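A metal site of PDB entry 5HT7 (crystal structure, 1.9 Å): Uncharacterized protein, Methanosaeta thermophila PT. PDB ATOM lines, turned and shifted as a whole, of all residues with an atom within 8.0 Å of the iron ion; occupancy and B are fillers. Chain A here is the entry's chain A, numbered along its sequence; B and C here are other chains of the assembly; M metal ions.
Of the 15 residues printed, 6 come within 4 Å of the iron ion.
The nearest printed residue that does not touch the iron ion is Val 3 of chain B (6.1 Å).
The iron ion is bound by NE2 of His 14 of chain A, NE2 of His 14 of chain B, NE2 of His 16 of chain A, NE2 of His 14 of chain C, NE2 of His 16 of chain B and NE2 of His 16 of chain C.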
ATOM      1  N   VAL A   3     -13.120  22.004 -21.379  1.00  0.00           N
ATOM      2  CA  VAL A   3     -11.842  21.686 -20.740  1.00  0.00           C
ATOM      3  C   VAL A   3     -11.085  22.965 -20.413  1.00  0.00           C
ATOM      4  O   VAL A   3     -10.942  23.828 -21.262  1.00  0.00           O
ATOM      5  CB  VAL A   3     -10.946  20.812 -21.638  1.00  0.00           C
ATOM      6  CG1 VAL A   3      -9.801  20.231 -20.819  1.00  0.00           C
ATOM      7  CG2 VAL A   3     -11.762  19.685 -22.255  1.00  0.00           C
ATOM      8  N   PHE A   5      -7.457  24.721 -18.981  1.00  0.00           N
ATOM      9  CA  PHE A   5      -6.028  24.442 -19.020  1.00  0.00           C
ATOM     10  C   PHE A   5      -5.270  25.495 -18.221  1.00  0.00           C
ATOM     11  O   PHE A   5      -5.579  26.690 -18.319  1.00  0.00           O
ATOM     12  CB  PHE A   5      -5.502  24.433 -20.471  1.00  0.00           C
ATOM     13  CG  PHE A   5      -6.063  23.326 -21.319  1.00  0.00           C
ATOM     14  CD1 PHE A   5      -5.414  22.116 -21.428  1.00  0.00           C
ATOM     15  CD2 PHE A   5      -7.250  23.496 -22.006  1.00  0.00           C
ATOM     16  CE1 PHE A   5      -5.932  21.083 -22.188  1.00  0.00           C
ATOM     17  CE2 PHE A   5      -7.778  22.479 -22.788  1.00  0.00           C
ATOM     18  CZ  PHE A   5      -7.111  21.263 -22.871  1.00  0.00           C
ATOM     19  N   HIS A  14      -4.904  20.077 -16.818  1.00  0.00           N
ATOM     20  CA  HIS A  14      -6.206  20.399 -17.369  1.00  0.00           C
ATOM     21  C   HIS A  14      -7.306  19.852 -16.476  1.00  0.00           C
ATOM     22  O   HIS A  14      -7.057  18.995 -15.615  1.00  0.00           O
ATOM     23  CB  HIS A  14      -6.329  19.858 -18.803  1.00  0.00           C
ATOM     24  CG  HIS A  14      -6.416  18.373 -18.879  1.00  0.00           C
ATOM     25  ND1 HIS A  14      -5.316  17.559 -18.970  1.00  0.00           N
ATOM     26  CD2 HIS A  14      -7.490  17.547 -18.915  1.00  0.00           C
ATOM     27  CE1 HIS A  14      -5.691  16.296 -19.047  1.00  0.00           C
ATOM     28  NE2 HIS A  14      -7.013  16.259 -18.995  1.00  0.00           N
ATOM     29  N   LYS A  15      -8.517  20.347 -16.688  1.00  0.00           N
ATOM     30  CA  LYS A  15      -9.670  20.021 -15.885  1.00  0.00           C
ATOM     31  C   LYS A  15     -10.908  19.905 -16.771  1.00  0.00           C
ATOM     32  O   LYS A  15     -11.231  20.829 -17.494  1.00  0.00           O
ATOM     33  CB  LYS A  15      -9.881  21.102 -14.817  1.00  0.00           C
ATOM     34  CG  LYS A  15     -11.072  20.875 -13.885  1.00  0.00           C
ATOM     35  CD  LYS A  15     -11.098  21.951 -12.793  1.00  0.00           C
ATOM     36  CE  LYS A  15     -12.461  21.980 -12.119  1.00  0.00           C
ATOM     37  NZ  LYS A  15     -12.794  20.693 -11.463  1.00  0.00           N
ATOM     38  N   HIS A  16     -11.575  18.756 -16.697  1.00  0.00           N
ATOM     39  CA  HIS A  16     -12.813  18.535 -17.448  1.00  0.00           C
ATOM     40  C   HIS A  16     -14.024  19.003 -16.686  1.00  0.00           C
ATOM     41  O   HIS A  16     -14.173  18.685 -15.501  1.00  0.00           O
ATOM     42  CB  HIS A  16     -12.985  17.047 -17.744  1.00  0.00           C
ATOM     43  CG  HIS A  16     -11.894  16.482 -18.588  1.00  0.00           C
ATOM     44  ND1 HIS A  16     -11.910  16.568 -19.960  1.00  0.00           N
ATOM     45  CD2 HIS A  16     -10.745  15.856 -18.265  1.00  0.00           C
ATOM     46  CE1 HIS A  16     -10.824  15.999 -20.449  1.00  0.00           C
ATOM     47  NE2 HIS A  16     -10.091  15.563 -19.443  1.00  0.00           N
ATOM     48  N   VAL B   3      -6.013  11.490 -27.818  1.00  0.00           N
ATOM     49  CA  VAL B   3      -5.453  11.535 -26.466  1.00  0.00           C
ATOM     50  C   VAL B   3      -4.129  10.782 -26.443  1.00  0.00           C
ATOM     51  O   VAL B   3      -4.072   9.607 -26.836  1.00  0.00           O
ATOM     52  CB  VAL B   3      -6.385  10.909 -25.403  1.00  0.00           C
ATOM     53  CG1 VAL B   3      -5.875  11.238 -23.989  1.00  0.00           C
ATOM     54  CG2 VAL B   3      -7.861  11.374 -25.576  1.00  0.00           C
ATOM     55  N   PHE B   5      -0.956   9.141 -24.221  1.00  0.00           N
ATOM     56  CA  PHE B   5      -0.668   8.644 -22.864  1.00  0.00           C
ATOM     57  C   PHE B   5       0.826   8.334 -22.701  1.00  0.00           C
ATOM     58  O   PHE B   5       1.459   7.803 -23.613  1.00  0.00           O
ATOM     59  CB  PHE B   5      -1.480   7.377 -22.549  1.00  0.00           C
ATOM     60  CG  PHE B   5      -2.950   7.601 -22.507  1.00  0.00           C
ATOM     61  CD1 PHE B   5      -3.597   7.863 -21.318  1.00  0.00           C
ATOM     62  CD2 PHE B   5      -3.693   7.575 -23.686  1.00  0.00           C
ATOM     63  CE1 PHE B   5      -4.959   8.082 -21.277  1.00  0.00           C
ATOM     64  CE2 PHE B   5      -5.063   7.811 -23.666  1.00  0.00           C
ATOM     65  CZ  PHE B   5      -5.700   8.066 -22.459  1.00  0.00           C
ATOM     66  N   HIS B  14      -1.629  12.043 -19.292  1.00  0.00           N
ATOM     67  CA  HIS B  14      -2.175  12.073 -20.641  1.00  0.00           C
ATOM     68  C   HIS B  14      -2.363  13.506 -21.122  1.00  0.00           C
ATOM     69  O   HIS B  14      -2.273  14.448 -20.330  1.00  0.00           O
ATOM     70  CB  HIS B  14      -3.497  11.302 -20.692  1.00  0.00           C
ATOM     71  CG  HIS B  14      -4.605  11.954 -19.925  1.00  0.00           C
ATOM     72  ND1 HIS B  14      -4.825  11.731 -18.581  1.00  0.00           N
ATOM     73  CD2 HIS B  14      -5.556  12.831 -20.324  1.00  0.00           C
ATOM     74  CE1 HIS B  14      -5.857  12.439 -18.185  1.00  0.00           C
ATOM     75  NE2 HIS B  14      -6.311  13.123 -19.218  1.00  0.00           N
ATOM     76  N   LYS B  15      -2.590  13.660 -22.420  1.00  0.00           N
ATOM     77  CA  LYS B  15      -2.668  14.975 -23.065  1.00  0.00           C
ATOM     78  C   LYS B  15      -3.719  14.948 -24.156  1.00  0.00           C
ATOM     79  O   LYS B  15      -3.704  14.056 -25.007  1.00  0.00           O
ATOM     80  CB  LYS B  15      -1.312  15.385 -23.642  1.00  0.00           C
ATOM     81  CG  LYS B  15      -1.318  16.724 -24.420  1.00  0.00           C
ATOM     82  CD  LYS B  15       0.117  17.149 -24.774  1.00  0.00           C
ATOM     83  CE  LYS B  15       0.175  18.370 -25.687  1.00  0.00           C
ATOM     84  NZ  LYS B  15      -0.515  19.570 -25.110  1.00  0.00           N
ATOM     85  N   HIS B  16      -4.635  15.917 -24.114  1.00  0.00           N
ATOM     86  CA  HIS B  16      -5.691  16.017 -25.124  1.00  0.00           C
ATOM     87  C   HIS B  16      -5.280  16.876 -26.292  1.00  0.00           C
ATOM     88  O   HIS B  16      -4.781  17.999 -26.092  1.00  0.00           O
ATOM     89  CB  HIS B  16      -6.959  16.592 -24.501  1.00  0.00           C
ATOM     90  CG  HIS B  16      -7.498  15.733 -23.421  1.00  0.00           C
ATOM     91  ND1 HIS B  16      -8.303  14.645 -23.676  1.00  0.00           N
ATOM     92  CD2 HIS B  16      -7.329  15.772 -22.082  1.00  0.00           C
ATOM     93  CE1 HIS B  16      -8.631  14.069 -22.540  1.00  0.00           C
ATOM     94  NE2 HIS B  16      -8.040  14.725 -21.565  1.00  0.00           N
ATOM     95  N   VAL C   3     -15.176   8.609 -17.215  1.00  0.00           N
ATOM     96  CA  VAL C   3     -14.098   9.308 -16.546  1.00  0.00           C
ATOM     97  C   VAL C   3     -14.222   9.074 -15.043  1.00  0.00           C
ATOM     98  O   VAL C   3     -15.296   9.260 -14.460  1.00  0.00           O
ATOM     99  CB  VAL C   3     -14.112  10.839 -16.844  1.00  0.00           C
ATOM    100  CG1 VAL C   3     -12.831  11.496 -16.310  1.00  0.00           C
ATOM    101  CG2 VAL C   3     -14.256  11.105 -18.353  1.00  0.00           C
ATOM    102  N   PHE C   5     -12.874  10.091 -11.183  1.00  0.00           N
ATOM    103  CA  PHE C   5     -12.257  11.224 -10.470  1.00  0.00           C
ATOM    104  C   PHE C   5     -11.883  10.830  -9.041  1.00  0.00           C
ATOM    105  O   PHE C   5     -12.637  10.105  -8.380  1.00  0.00           O
ATOM    106  CB  PHE C   5     -13.191  12.426 -10.429  1.00  0.00           C
ATOM    107  CG  PHE C   5     -13.524  12.994 -11.769  1.00  0.00           C
ATOM    108  CD1 PHE C   5     -12.791  14.043 -12.293  1.00  0.00           C
ATOM    109  CD2 PHE C   5     -14.590  12.496 -12.504  1.00  0.00           C
ATOM    110  CE1 PHE C   5     -13.107  14.576 -13.537  1.00  0.00           C
ATOM    111  CE2 PHE C   5     -14.914  13.019 -13.751  1.00  0.00           C
ATOM    112  CZ  PHE C   5     -14.170  14.061 -14.257  1.00  0.00           C
ATOM    113  N   HIS C  14      -7.898  12.674 -12.518  1.00  0.00           N
ATOM    114  CA  HIS C  14      -8.928  11.906 -13.221  1.00  0.00           C
ATOM    115  C   HIS C  14      -8.297  10.888 -14.160  1.00  0.00           C
ATOM    116  O   HIS C  14      -7.086  10.937 -14.439  1.00  0.00           O
ATOM    117  CB  HIS C  14      -9.853  12.839 -14.001  1.00  0.00           C
ATOM    118  CG  HIS C  14      -9.178  13.509 -15.150  1.00  0.00           C
ATOM    119  ND1 HIS C  14      -8.371  14.618 -14.993  1.00  0.00           N
ATOM    120  CD2 HIS C  14      -9.168  13.217 -16.466  1.00  0.00           C
ATOM    121  CE1 HIS C  14      -7.888  14.976 -16.172  1.00  0.00           C
ATOM    122  NE2 HIS C  14      -8.350  14.140 -17.077  1.00  0.00           N
ATOM    123  N   LYS C  15      -9.110   9.963 -14.632  1.00  0.00           N
ATOM    124  CA  LYS C  15      -8.617   8.885 -15.495  1.00  0.00           C
ATOM    125  C   LYS C  15      -9.669   8.556 -16.545  1.00  0.00           C
ATOM    126  O   LYS C  15     -10.832   8.347 -16.221  1.00  0.00           O
ATOM    127  CB  LYS C  15      -8.308   7.634 -14.661  1.00  0.00           C
ATOM    128  CG  LYS C  15      -7.945   6.380 -15.465  1.00  0.00           C
ATOM    129  CD  LYS C  15      -7.404   5.293 -14.524  1.00  0.00           C
ATOM    130  CE  LYS C  15      -7.210   3.968 -15.248  1.00  0.00           C
ATOM    131  NZ  LYS C  15      -6.195   4.040 -16.311  1.00  0.00           N
ATOM    132  N   HIS C  16      -9.270   8.492 -17.808  1.00  0.00           N
ATOM    133  CA  HIS C  16     -10.212   8.163 -18.877  1.00  0.00           C
ATOM    134  C   HIS C  16     -10.286   6.679 -19.125  1.00  0.00           C
ATOM    135  O   HIS C  16      -9.243   6.018 -19.282  1.00  0.00           O
ATOM    136  CB  HIS C  16      -9.811   8.873 -20.164  1.00  0.00           C
ATOM    137  CG  HIS C  16      -9.831  10.356 -20.047  1.00  0.00           C
ATOM    138  ND1 HIS C  16     -10.976  11.095 -20.201  1.00  0.00           N
ATOM    139  CD2 HIS C  16      -8.852  11.228 -19.730  1.00  0.00           C
ATOM    140  CE1 HIS C  16     -10.706  12.366 -20.018  1.00  0.00           C
ATOM    141  NE2 HIS C  16      -9.423  12.481 -19.724  1.00  0.00           N
HETATM  142 FE    FE M   1      -8.170  14.369 -19.327  1.00  0.00          FE
